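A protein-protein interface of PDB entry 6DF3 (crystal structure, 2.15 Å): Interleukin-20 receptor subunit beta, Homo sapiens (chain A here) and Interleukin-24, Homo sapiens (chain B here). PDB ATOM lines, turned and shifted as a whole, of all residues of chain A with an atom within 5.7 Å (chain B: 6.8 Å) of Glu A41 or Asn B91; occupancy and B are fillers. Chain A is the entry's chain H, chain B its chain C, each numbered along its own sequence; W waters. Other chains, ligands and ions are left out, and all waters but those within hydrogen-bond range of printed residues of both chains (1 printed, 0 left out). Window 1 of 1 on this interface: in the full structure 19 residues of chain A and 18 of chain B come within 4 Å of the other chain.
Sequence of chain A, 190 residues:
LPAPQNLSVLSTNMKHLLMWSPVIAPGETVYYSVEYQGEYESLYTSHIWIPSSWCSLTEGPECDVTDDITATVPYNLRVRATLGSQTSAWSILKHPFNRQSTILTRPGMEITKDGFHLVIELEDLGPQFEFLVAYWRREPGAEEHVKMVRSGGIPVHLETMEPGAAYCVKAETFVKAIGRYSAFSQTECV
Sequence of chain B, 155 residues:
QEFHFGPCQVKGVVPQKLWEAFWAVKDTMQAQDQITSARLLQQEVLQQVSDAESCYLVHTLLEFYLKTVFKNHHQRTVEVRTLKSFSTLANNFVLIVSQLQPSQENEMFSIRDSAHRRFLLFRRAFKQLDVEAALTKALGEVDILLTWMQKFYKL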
ATOM      1  N   GLN A  37      14.462 -26.550 -16.036  1.00  0.00           N
ATOM      2  CA  GLN A  37      13.253 -26.918 -15.319  1.00  0.00           C
ATOM      3  C   GLN A  37      13.513 -28.232 -14.628  1.00  0.00           C
ATOM      4  O   GLN A  37      14.083 -29.168 -15.231  1.00  0.00           O
ATOM      5  CB  GLN A  37      12.140 -27.311 -16.298  1.00  0.00           C
ATOM      6  CG  GLN A  37      11.707 -26.174 -17.160  1.00  0.00           C
ATOM      7  CD  GLN A  37      10.494 -26.498 -18.017  1.00  0.00           C
ATOM      8  OE1 GLN A  37      10.428 -27.571 -18.606  1.00  0.00           O
ATOM      9  NE2 GLN A  37       9.595 -25.555 -18.151  1.00  0.00           N
ATOM     10  N   GLY A  38      13.103 -28.343 -13.383  1.00  0.00           N
ATOM     11  CA  GLY A  38      13.049 -29.669 -12.745  1.00  0.00           C
ATOM     12  C   GLY A  38      11.793 -30.315 -13.237  1.00  0.00           C
ATOM     13  O   GLY A  38      11.005 -29.694 -13.958  1.00  0.00           O
ATOM     14  N   GLU A  39      11.597 -31.551 -12.854  1.00  0.00           N
ATOM     15  CA  GLU A  39      10.373 -32.265 -13.142  1.00  0.00           C
ATOM     16  C   GLU A  39       9.111 -31.563 -12.606  1.00  0.00           C
ATOM     17  O   GLU A  39       8.038 -31.694 -13.188  1.00  0.00           O
ATOM     18  CB  GLU A  39      10.449 -33.650 -12.525  1.00  0.00           C
ATOM     19  CG  GLU A  39       9.301 -34.522 -12.940  1.00  0.00           C
ATOM     20  CD  GLU A  39       9.329 -35.935 -12.321  1.00  0.00           C
ATOM     21  OE1 GLU A  39      10.021 -36.180 -11.291  1.00  0.00           O
ATOM     22  OE2 GLU A  39       8.666 -36.827 -12.912  1.00  0.00           O
ATOM     23  N   TYR A  40       9.195 -30.931 -11.431  1.00  0.00           N
ATOM     24  CA  TYR A  40       8.101 -30.191 -10.995  1.00  0.00           C
ATOM     25  C   TYR A  40       7.662 -29.200 -12.146  1.00  0.00           C
ATOM     26  O   TYR A  40       6.507 -29.202 -12.568  1.00  0.00           O
ATOM     27  CB  TYR A  40       8.406 -29.363  -9.753  1.00  0.00           C
ATOM     28  CG  TYR A  40       7.206 -28.500  -9.372  1.00  0.00           C
ATOM     29  CD1 TYR A  40       6.017 -29.069  -8.946  1.00  0.00           C
ATOM     30  CD2 TYR A  40       7.236 -27.146  -9.526  1.00  0.00           C
ATOM     31  CE1 TYR A  40       4.902 -28.309  -8.585  1.00  0.00           C
ATOM     32  CE2 TYR A  40       6.115 -26.350  -9.204  1.00  0.00           C
ATOM     33  CZ  TYR A  40       4.955 -26.945  -8.762  1.00  0.00           C
ATOM     34  OH  TYR A  40       3.920 -26.159  -8.436  1.00  0.00           O
ATOM     35  N   GLU A  41       8.577 -28.365 -12.624  1.00  0.00           N
ATOM     36  CA  GLU A  41       8.199 -27.326 -13.546  1.00  0.00           C
ATOM     37  C   GLU A  41       7.720 -27.941 -14.885  1.00  0.00           C
ATOM     38  O   GLU A  41       6.710 -27.542 -15.464  1.00  0.00           O
ATOM     39  CB  GLU A  41       9.321 -26.343 -13.713  1.00  0.00           C
ATOM     40  CG  GLU A  41       9.601 -25.509 -12.443  1.00  0.00           C
ATOM     41  CD  GLU A  41      10.533 -26.136 -11.412  1.00  0.00           C
ATOM     42  OE1 GLU A  41      11.059 -27.260 -11.643  1.00  0.00           O
ATOM     43  OE2 GLU A  41      10.602 -25.580 -10.312  1.00  0.00           O
ATOM     44  N   SER A  42       8.404 -29.005 -15.270  1.00  0.00           N
ATOM     45  CA  SER A  42       8.124 -29.798 -16.415  1.00  0.00           C
ATOM     46  C   SER A  42       6.660 -30.270 -16.432  1.00  0.00           C
ATOM     47  O   SER A  42       5.992 -30.126 -17.426  1.00  0.00           O
ATOM     48  CB  SER A  42       9.064 -30.987 -16.412  1.00  0.00           C
ATOM     49  OG  SER A  42       9.234 -31.405 -17.717  1.00  0.00           O
ATOM     50  N   LEU A  43       6.180 -30.804 -15.323  1.00  0.00           N
ATOM     51  CA  LEU A  43       4.800 -31.299 -15.172  1.00  0.00           C
ATOM     52  C   LEU A  43       3.724 -30.290 -14.717  1.00  0.00           C
ATOM     53  O   LEU A  43       2.574 -30.512 -14.976  1.00  0.00           O
ATOM     54  CB  LEU A  43       4.763 -32.441 -14.145  1.00  0.00           C
ATOM     55  CG  LEU A  43       5.501 -33.722 -14.486  1.00  0.00           C
ATOM     56  CD1 LEU A  43       5.628 -34.627 -13.280  1.00  0.00           C
ATOM     57  CD2 LEU A  43       4.786 -34.490 -15.611  1.00  0.00           C
ATOM     58  N   TYR A  44       4.044 -29.249 -13.980  1.00  0.00           N
ATOM     59  CA  TYR A  44       2.985 -28.457 -13.395  1.00  0.00           C
ATOM     60  C   TYR A  44       3.029 -27.001 -13.893  1.00  0.00           C
ATOM     61  O   TYR A  44       2.068 -26.308 -13.710  1.00  0.00           O
ATOM     62  CB  TYR A  44       3.070 -28.450 -11.835  1.00  0.00           C
ATOM     63  CG  TYR A  44       2.744 -29.740 -11.026  1.00  0.00           C
ATOM     64  CD1 TYR A  44       3.685 -30.755 -10.896  1.00  0.00           C
ATOM     65  CD2 TYR A  44       1.561 -29.890 -10.350  1.00  0.00           C
ATOM     66  CE1 TYR A  44       3.430 -31.917 -10.172  1.00  0.00           C
ATOM     67  CE2 TYR A  44       1.289 -31.072  -9.635  1.00  0.00           C
ATOM     68  CZ  TYR A  44       2.262 -32.072  -9.547  1.00  0.00           C
ATOM     69  OH  TYR A  44       2.099 -33.239  -8.785  1.00  0.00           O
ATOM     70  N   THR A  45       4.163 -26.523 -14.427  1.00  0.00           N
ATOM     71  CA  THR A  45       4.353 -25.138 -14.836  1.00  0.00           C
ATOM     72  C   THR A  45       5.291 -25.185 -16.064  1.00  0.00           C
ATOM     73  O   THR A  45       6.403 -24.611 -16.059  1.00  0.00           O
ATOM     74  CB  THR A  45       4.925 -24.211 -13.702  1.00  0.00           C
ATOM     75  OG1 THR A  45       6.248 -24.583 -13.233  1.00  0.00           O
ATOM     76  CG2 THR A  45       4.047 -24.191 -12.547  1.00  0.00           C
ATOM     77  N   SER A  46       4.863 -25.894 -17.114  1.00  0.00           N
ATOM     78  CA  SER A  46       5.763 -26.242 -18.204  1.00  0.00           C
ATOM     79  C   SER A  46       6.282 -25.057 -19.002  1.00  0.00           C
ATOM     80  O   SER A  46       7.289 -25.172 -19.714  1.00  0.00           O
ATOM     81  CB  SER A  46       5.125 -27.289 -19.123  1.00  0.00           C
ATOM     82  OG  SER A  46       3.902 -26.831 -19.730  1.00  0.00           O
ATOM     83  N   HIS A  47       5.670 -23.895 -18.798  1.00  0.00           N
ATOM     84  CA  HIS A  47       6.057 -22.696 -19.495  1.00  0.00           C
ATOM     85  C   HIS A  47       7.118 -21.911 -18.767  1.00  0.00           C
ATOM     86  O   HIS A  47       7.564 -20.837 -19.225  1.00  0.00           O
ATOM     87  CB  HIS A  47       4.776 -21.873 -19.771  1.00  0.00           C
ATOM     88  CG  HIS A  47       4.087 -21.413 -18.512  1.00  0.00           C
ATOM     89  ND1 HIS A  47       3.439 -22.290 -17.654  1.00  0.00           N
ATOM     90  CD2 HIS A  47       4.023 -20.191 -17.925  1.00  0.00           C
ATOM     91  CE1 HIS A  47       2.977 -21.619 -16.618  1.00  0.00           C
ATOM     92  NE2 HIS A  47       3.290 -20.339 -16.768  1.00  0.00           N
ATOM     93  N   ILE A  48       7.591 -22.407 -17.641  1.00  0.00           N
ATOM     94  CA  ILE A  48       8.508 -21.597 -16.819  1.00  0.00           C
ATOM     95  C   ILE A  48       9.881 -22.267 -16.816  1.00  0.00           C
ATOM     96  O   ILE A  48       9.989 -23.429 -16.377  1.00  0.00           O
ATOM     97  CB  ILE A  48       8.014 -21.473 -15.366  1.00  0.00           C
ATOM     98  CG1 ILE A  48       6.728 -20.657 -15.319  1.00  0.00           C
ATOM     99  CG2 ILE A  48       9.118 -20.887 -14.473  1.00  0.00           C
ATOM    100  CD1 ILE A  48       6.060 -20.524 -13.953  1.00  0.00           C
ATOM    101  N   ILE A  50      13.919 -21.538 -15.486  1.00  0.00           N
ATOM    102  CA  ILE A  50      14.630 -20.797 -14.457  1.00  0.00           C
ATOM    103  C   ILE A  50      16.081 -20.518 -14.890  1.00  0.00           C
ATOM    104  O   ILE A  50      16.778 -21.403 -15.381  1.00  0.00           O
ATOM    105  CB  ILE A  50      14.646 -21.654 -13.183  1.00  0.00           C
ATOM    106  CG1 ILE A  50      13.215 -22.037 -12.863  1.00  0.00           C
ATOM    107  CG2 ILE A  50      15.396 -20.963 -12.044  1.00  0.00           C
ATOM    108  CD1 ILE A  50      13.154 -23.163 -11.894  1.00  0.00           C
ATOM    109  N   ALA A  71      17.528 -31.792  -6.782  1.00  0.00           N
ATOM    110  CA  ALA A  71      16.735 -32.932  -6.448  1.00  0.00           C
ATOM    111  C   ALA A  71      17.066 -34.144  -7.380  1.00  0.00           C
ATOM    112  O   ALA A  71      17.430 -33.999  -8.558  1.00  0.00           O
ATOM    113  CB  ALA A  71      15.284 -32.557  -6.549  1.00  0.00           C
ATOM    114  N   VAL A  73      15.534 -36.001  -9.507  1.00  0.00           N
ATOM    115  CA  VAL A  73      14.464 -36.090 -10.465  1.00  0.00           C
ATOM    116  C   VAL A  73      15.058 -35.615 -11.834  1.00  0.00           C
ATOM    117  O   VAL A  73      16.154 -34.960 -11.863  1.00  0.00           O
ATOM    118  CB  VAL A  73      13.260 -35.183 -10.064  1.00  0.00           C
ATOM    119  CG1 VAL A  73      12.729 -35.493  -8.665  1.00  0.00           C
ATOM    120  CG2 VAL A  73      13.611 -33.706 -10.129  1.00  0.00           C
ATOM    121  N   PRO A  74      14.375 -35.950 -12.969  1.00  0.00           N
ATOM    122  CA  PRO A  74      14.879 -35.494 -14.259  1.00  0.00           C
ATOM    123  C   PRO A  74      14.661 -34.013 -14.457  1.00  0.00           C
ATOM    124  O   PRO A  74      13.601 -33.528 -14.135  1.00  0.00           O
ATOM    125  CB  PRO A  74      14.048 -36.288 -15.331  1.00  0.00           C
ATOM    126  CG  PRO A  74      12.858 -36.826 -14.560  1.00  0.00           C
ATOM    127  CD  PRO A  74      13.189 -36.826 -13.077  1.00  0.00           C
ATOM    128  N   TYR A  75      15.640 -33.359 -15.079  1.00  0.00           N
ATOM    129  CA  TYR A  75      15.705 -31.947 -15.341  1.00  0.00           C
ATOM    130  C   TYR A  75      15.844 -31.731 -16.870  1.00  0.00           C
ATOM    131  O   TYR A  75      16.614 -32.403 -17.519  1.00  0.00           O
ATOM    132  CB  TYR A  75      16.958 -31.335 -14.645  1.00  0.00           C
ATOM    133  CG  TYR A  75      16.754 -30.899 -13.245  1.00  0.00           C
ATOM    134  CD1 TYR A  75      16.799 -31.828 -12.225  1.00  0.00           C
ATOM    135  CD2 TYR A  75      16.528 -29.562 -12.922  1.00  0.00           C
ATOM    136  CE1 TYR A  75      16.598 -31.457 -10.877  1.00  0.00           C
ATOM    137  CE2 TYR A  75      16.313 -29.168 -11.578  1.00  0.00           C
ATOM    138  CZ  TYR A  75      16.351 -30.114 -10.544  1.00  0.00           C
ATOM    139  OH  TYR A  75      16.222 -29.803  -9.188  1.00  0.00           O
ATOM    140  N   VAL B  13      15.932 -38.079  -0.419  1.00  0.00           N
ATOM    141  CA  VAL B  13      15.530 -36.643  -0.024  1.00  0.00           C
ATOM    142  C   VAL B  13      16.232 -36.379   1.327  1.00  0.00           C
ATOM    143  O   VAL B  13      16.009 -37.121   2.300  1.00  0.00           O
ATOM    144  CB  VAL B  13      14.016 -36.495   0.116  1.00  0.00           C
ATOM    145  CG1 VAL B  13      13.610 -35.097   0.589  1.00  0.00           C
ATOM    146  CG2 VAL B  13      13.329 -36.776  -1.216  1.00  0.00           C
ATOM    147  N   LEU B  66       2.130 -28.738  -4.068  1.00  0.00           N
ATOM    148  CA  LEU B  66       2.468 -28.847  -5.477  1.00  0.00           C
ATOM    149  C   LEU B  66       1.466 -28.203  -6.434  1.00  0.00           C
ATOM    150  O   LEU B  66       1.863 -27.468  -7.314  1.00  0.00           O
ATOM    151  CB  LEU B  66       2.605 -30.312  -5.894  1.00  0.00           C
ATOM    152  CG  LEU B  66       3.719 -31.022  -5.199  1.00  0.00           C
ATOM    153  CD1 LEU B  66       3.747 -32.477  -5.692  1.00  0.00           C
ATOM    154  CD2 LEU B  66       5.058 -30.337  -5.413  1.00  0.00           C
ATOM    155  N   PHE B  70       2.837 -23.860  -4.632  1.00  0.00           N
ATOM    156  CA  PHE B  70       4.044 -23.627  -5.463  1.00  0.00           C
ATOM    157  C   PHE B  70       3.761 -23.235  -6.887  1.00  0.00           C
ATOM    158  O   PHE B  70       4.510 -22.499  -7.479  1.00  0.00           O
ATOM    159  CB  PHE B  70       4.948 -24.839  -5.443  1.00  0.00           C
ATOM    160  CG  PHE B  70       5.574 -25.137  -4.100  1.00  0.00           C
ATOM    161  CD1 PHE B  70       5.776 -24.180  -3.145  1.00  0.00           C
ATOM    162  CD2 PHE B  70       5.961 -26.398  -3.806  1.00  0.00           C
ATOM    163  CE1 PHE B  70       6.380 -24.479  -1.936  1.00  0.00           C
ATOM    164  CE2 PHE B  70       6.531 -26.725  -2.591  1.00  0.00           C
ATOM    165  CZ  PHE B  70       6.769 -25.749  -1.651  1.00  0.00           C
ATOM    166  N   HIS B  74       5.206 -19.820  -8.363  1.00  0.00           N
ATOM    167  CA  HIS B  74       6.014 -19.846  -9.601  1.00  0.00           C
ATOM    168  C   HIS B  74       5.461 -18.871 -10.602  1.00  0.00           C
ATOM    169  O   HIS B  74       6.200 -18.149 -11.243  1.00  0.00           O
ATOM    170  CB  HIS B  74       6.056 -21.255 -10.242  1.00  0.00           C
ATOM    171  CG  HIS B  74       7.190 -22.106  -9.780  1.00  0.00           C
ATOM    172  ND1 HIS B  74       7.726 -22.031  -8.517  1.00  0.00           N
ATOM    173  CD2 HIS B  74       7.845 -23.125 -10.403  1.00  0.00           C
ATOM    174  CE1 HIS B  74       8.627 -22.996  -8.363  1.00  0.00           C
ATOM    175  NE2 HIS B  74       8.756 -23.642  -9.514  1.00  0.00           N
ATOM    176  N   LEU B  83      12.256 -18.139  -6.730  1.00  0.00           N
ATOM    177  CA  LEU B  83      12.012 -19.087  -7.798  1.00  0.00           C
ATOM    178  C   LEU B  83      12.934 -20.329  -7.671  1.00  0.00           C
ATOM    179  O   LEU B  83      12.457 -21.435  -7.792  1.00  0.00           O
ATOM    180  CB  LEU B  83      12.159 -18.463  -9.139  1.00  0.00           C
ATOM    181  CG  LEU B  83      11.917 -19.384 -10.339  1.00  0.00           C
ATOM    182  CD1 LEU B  83      10.519 -19.949 -10.313  1.00  0.00           C
ATOM    183  CD2 LEU B  83      12.130 -18.592 -11.609  1.00  0.00           C
ATOM    184  N   LYS B  84      14.210 -20.117  -7.347  1.00  0.00           N
ATOM    185  CA  LYS B  84      15.181 -21.189  -7.243  1.00  0.00           C
ATOM    186  C   LYS B  84      14.954 -21.976  -5.994  1.00  0.00           C
ATOM    187  O   LYS B  84      14.948 -23.198  -6.045  1.00  0.00           O
ATOM    188  CB  LYS B  84      16.616 -20.682  -7.369  1.00  0.00           C
ATOM    189  CG  LYS B  84      16.912 -20.100  -8.737  1.00  0.00           C
ATOM    190  CD  LYS B  84      18.365 -19.559  -8.887  1.00  0.00           C
ATOM    191  CE  LYS B  84      19.253 -20.443  -9.829  1.00  0.00           C
ATOM    192  NZ  LYS B  84      19.377 -21.948  -9.490  1.00  0.00           N
ATOM    193  N   PHE B  86      12.136 -22.268  -4.038  1.00  0.00           N
ATOM    194  CA  PHE B  86      10.914 -23.068  -4.141  1.00  0.00           C
ATOM    195  C   PHE B  86      10.946 -24.140  -5.215  1.00  0.00           C
ATOM    196  O   PHE B  86      10.320 -25.190  -5.017  1.00  0.00           O
ATOM    197  CB  PHE B  86       9.677 -22.171  -4.143  1.00  0.00           C
ATOM    198  CG  PHE B  86       9.496 -21.473  -2.802  1.00  0.00           C
ATOM    199  CD1 PHE B  86       9.069 -22.203  -1.678  1.00  0.00           C
ATOM    200  CD2 PHE B  86       9.739 -20.144  -2.645  1.00  0.00           C
ATOM    201  CE1 PHE B  86       8.928 -21.607  -0.393  1.00  0.00           C
ATOM    202  CE2 PHE B  86       9.558 -19.558  -1.408  1.00  0.00           C
ATOM    203  CZ  PHE B  86       9.130 -20.299  -0.288  1.00  0.00           C
ATOM    204  N   SER B  87      11.790 -23.991  -6.248  1.00  0.00           N
ATOM    205  CA  SER B  87      11.963 -25.095  -7.264  1.00  0.00           C
ATOM    206  C   SER B  87      12.578 -26.272  -6.545  1.00  0.00           C
ATOM    207  O   SER B  87      12.064 -27.411  -6.624  1.00  0.00           O
ATOM    208  CB  SER B  87      12.788 -24.629  -8.436  1.00  0.00           C
ATOM    209  OG  SER B  87      12.959 -25.593  -9.434  1.00  0.00           O
ATOM    210  N   THR B  88      13.600 -25.997  -5.720  1.00  0.00           N
ATOM    211  CA  THR B  88      14.285 -27.045  -4.989  1.00  0.00           C
ATOM    212  C   THR B  88      13.291 -27.770  -4.096  1.00  0.00           C
ATOM    213  O   THR B  88      13.236 -29.026  -4.080  1.00  0.00           O
ATOM    214  CB  THR B  88      15.460 -26.471  -4.184  1.00  0.00           C
ATOM    215  OG1 THR B  88      16.436 -25.975  -5.122  1.00  0.00           O
ATOM    216  CG2 THR B  88      16.132 -27.553  -3.272  1.00  0.00           C
ATOM    217  N   LEU B  89      12.490 -27.013  -3.346  1.00  0.00           N
ATOM    218  CA  LEU B  89      11.531 -27.672  -2.468  1.00  0.00           C
ATOM    219  C   LEU B  89      10.453 -28.424  -3.305  1.00  0.00           C
ATOM    220  O   LEU B  89      10.107 -29.528  -2.977  1.00  0.00           O
ATOM    221  CB  LEU B  89      10.845 -26.680  -1.506  1.00  0.00           C
ATOM    222  CG  LEU B  89      11.801 -26.058  -0.493  1.00  0.00           C
ATOM    223  CD1 LEU B  89      11.270 -24.801   0.095  1.00  0.00           C
ATOM    224  CD2 LEU B  89      12.074 -27.050   0.638  1.00  0.00           C
ATOM    225  N   ALA B  90       9.967 -27.822  -4.369  1.00  0.00           N
ATOM    226  CA  ALA B  90       8.855 -28.438  -5.098  1.00  0.00           C
ATOM    227  C   ALA B  90       9.391 -29.735  -5.773  1.00  0.00           C
ATOM    228  O   ALA B  90       8.725 -30.760  -5.733  1.00  0.00           O
ATOM    229  CB  ALA B  90       8.360 -27.516  -6.145  1.00  0.00           C
ATOM    230  N   ASN B  91      10.597 -29.674  -6.328  1.00  0.00           N
ATOM    231  CA  ASN B  91      11.189 -30.871  -6.903  1.00  0.00           C
ATOM    232  C   ASN B  91      11.437 -31.994  -5.955  1.00  0.00           C
ATOM    233  O   ASN B  91      11.138 -33.108  -6.249  1.00  0.00           O
ATOM    234  CB  ASN B  91      12.395 -30.506  -7.747  1.00  0.00           C
ATOM    235  CG  ASN B  91      11.953 -29.929  -9.084  1.00  0.00           C
ATOM    236  OD1 ASN B  91      11.456 -30.720  -9.902  1.00  0.00           O
ATOM    237  ND2 ASN B  91      12.081 -28.552  -9.304  1.00  0.00           N
ATOM    238  N   ASN B  92      11.900 -31.698  -4.754  1.00  0.00           N
ATOM    239  CA  ASN B  92      12.051 -32.738  -3.744  1.00  0.00           C
ATOM    240  C   ASN B  92      10.660 -33.225  -3.271  1.00  0.00           C
ATOM    241  O   ASN B  92      10.501 -34.403  -2.976  1.00  0.00           O
ATOM    242  CB  ASN B  92      12.867 -32.182  -2.561  1.00  0.00           C
ATOM    243  CG  ASN B  92      14.345 -32.266  -2.827  1.00  0.00           C
ATOM    244  OD1 ASN B  92      14.924 -33.350  -2.671  1.00  0.00           O
ATOM    245  ND2 ASN B  92      14.953 -31.176  -3.277  1.00  0.00           N
ATOM    246  N   PHE B  93       9.688 -32.336  -3.165  1.00  0.00           N
ATOM    247  CA  PHE B  93       8.296 -32.787  -2.822  1.00  0.00           C
ATOM    248  C   PHE B  93       7.692 -33.740  -3.864  1.00  0.00           C
ATOM    249  O   PHE B  93       7.065 -34.774  -3.480  1.00  0.00           O
ATOM    250  CB  PHE B  93       7.336 -31.643  -2.615  1.00  0.00           C
ATOM    251  CG  PHE B  93       7.530 -30.852  -1.318  1.00  0.00           C
ATOM    252  CD1 PHE B  93       8.669 -30.997  -0.485  1.00  0.00           C
ATOM    253  CD2 PHE B  93       6.593 -29.907  -0.957  1.00  0.00           C
ATOM    254  CE1 PHE B  93       8.788 -30.250   0.711  1.00  0.00           C
ATOM    255  CE2 PHE B  93       6.747 -29.099   0.208  1.00  0.00           C
ATOM    256  CZ  PHE B  93       7.857 -29.255   1.010  1.00  0.00           C
ATOM    257  N   VAL B  94       7.956 -33.472  -5.139  1.00  0.00           N
ATOM    258  CA  VAL B  94       7.620 -34.408  -6.219  1.00  0.00           C
ATOM    259  C   VAL B  94       8.267 -35.782  -5.950  1.00  0.00           C
ATOM    260  O   VAL B  94       7.604 -36.804  -6.033  1.00  0.00           O
ATOM    261  CB  VAL B  94       8.016 -33.891  -7.632  1.00  0.00           C
ATOM    262  CG1 VAL B  94       7.899 -35.016  -8.671  1.00  0.00           C
ATOM    263  CG2 VAL B  94       7.090 -32.744  -8.034  1.00  0.00           C
ATOM    264  N   LEU B  95       9.531 -35.799  -5.555  1.00  0.00           N
ATOM    265  CA  LEU B  95      10.192 -37.072  -5.359  1.00  0.00           C
ATOM    266  C   LEU B  95       9.550 -37.823  -4.143  1.00  0.00           C
ATOM    267  O   LEU B  95       9.324 -39.031  -4.179  1.00  0.00           O
ATOM    268  CB  LEU B  95      11.678 -36.830  -5.204  1.00  0.00           C
ATOM    269  CG  LEU B  95      12.550 -38.063  -4.969  1.00  0.00           C
ATOM    270  CD1 LEU B  95      12.466 -39.233  -5.962  1.00  0.00           C
ATOM    271  CD2 LEU B  95      13.983 -37.549  -4.911  1.00  0.00           C
ATOM    272  N   ILE B  96       9.177 -37.078  -3.101  1.00  0.00           N
ATOM    273  CA  ILE B  96       8.523 -37.689  -1.896  1.00  0.00           C
ATOM    274  C   ILE B  96       7.211 -38.328  -2.317  1.00  0.00           C
ATOM    275  O   ILE B  96       6.999 -39.501  -2.067  1.00  0.00           O
ATOM    276  CB  ILE B  96       8.249 -36.705  -0.759  1.00  0.00           C
ATOM    277  CG1 ILE B  96       9.577 -36.210  -0.213  1.00  0.00           C
ATOM    278  CG2 ILE B  96       7.406 -37.403   0.328  1.00  0.00           C
ATOM    279  CD1 ILE B  96       9.480 -35.086   0.789  1.00  0.00           C
HETATM  280  O   HOH W   1      15.238 -27.361  -8.706  1.00  0.00           O
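The backbone carbonyl oxygen (O) of Phe B70 sits close to a ring nitrogen (ND1) of His B74, 3.4 Å away.
The backbone carbonyl oxygen (O) of Lys B84 lies within hydrogen-bond range of the side-chain hydroxyl (OG1) of Thr B88 (3.3 Å).
ND2 of Asn B91 is in hydrogen-bond range of O of Ser B87.
The side-chain amide nitrogen (NE2) of Gln A37 sits at hydrogen-bond distance from the backbone carbonyl oxygen (O) of Ile A48 (2.8 Å).
O of Glu A41 lies within hydrogen-bond range of N of Ser A46 (3.0 Å).
N of Ala A71 lies within hydrogen-bond range of OH of Tyr A75.
Asn B91 touches Gly A38 (OD1 to C, 3.4 Å).
Tyr A40 touches Ala B90 (CG to CB, 3.6 Å).
CD1 of Tyr A40 touches CG2 of Val B94, 3.9 Å away.
Tyr A44 touches Leu B66 (OH to CD1, 3.6 Å).
Thr A45 touches His B74.
Leu B83 touches Ile A50 (CD2 to CG1, 3.8 Å).
Ile A50 touches Ser B87 (CD1 to OG, 3.5 Å).
Ala A71 touches Asn B91.
Asn B91 touches Val A73 (OD1 to CG2, 3.7 Å).
CG1 of Val A73 touches CB of Leu B95, 3.9 Å away.
Hydrophobic or aromatic side chains of chain B within 4 Å of the printed part of chain A: Leu B66, Phe B70, His B74, Leu B83, Ala B90, Val B94 and Leu B95.
Of the 17 printed residues of chain A, 10 touch a printed residue of chain B.
Among the printed residues, 22 pairs touch across the chains.
Glu A41 touches just these residues of chain B: His B74 (2.8 Å), Ser B87 (2.5 Å) and Asn B91 (2.9 Å).
Of the printed residues of chain A, His B74 touches Tyr A40, Glu A41, Thr A45 and Ile A48.
Leu B89 touches none of the printed residues of chain A.
Asn B91 touches just these residues of chain A: Gly A38 (3.4 Å), Glu A39 (3.1 Å), Tyr A40 (2.7 Å), Glu A41 (2.9 Å), Ala A71 (3.7 Å) and Val A73 (3.7 Å).
Of the printed residues of chain A, Asn B92 touches Ala A71 (3.6 Å).
Printed residues of chain A within 4 Å of Leu B95: Val A73.
The nearest residue of chain A that does not touch Asn B91 is Tyr A75 (4.1 Å).
O of Leu B66 lies within hydrogen-bond range of OH of Tyr A40.
NE2 of His B74 is in hydrogen-bond range of OE2 of Glu A41 (2.8 Å).
The side-chain carboxylate (OE2) of Glu A41 sits at hydrogen-bond distance from the side-chain hydroxyl (OG) of Ser B87.
The backbone NH of Glu A39 is in hydrogen-bond range of the side-chain amide oxygen of Asn B91 (3.1 Å).
N of Tyr A40 sits at hydrogen-bond distance from OD1 of Asn B91 (2.7 Å).
The side-chain amide nitrogen (ND2) of Asn B91 sits at hydrogen-bond distance from the side-chain carboxylate (OE1) of Glu A41 (2.9 Å).
Water W1 lies within hydrogen-bond range of the side-chain hydroxyl of Tyr A75, the side-chain hydroxyl of Ser B87 and the side-chain amide nitrogen of Asn B91.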
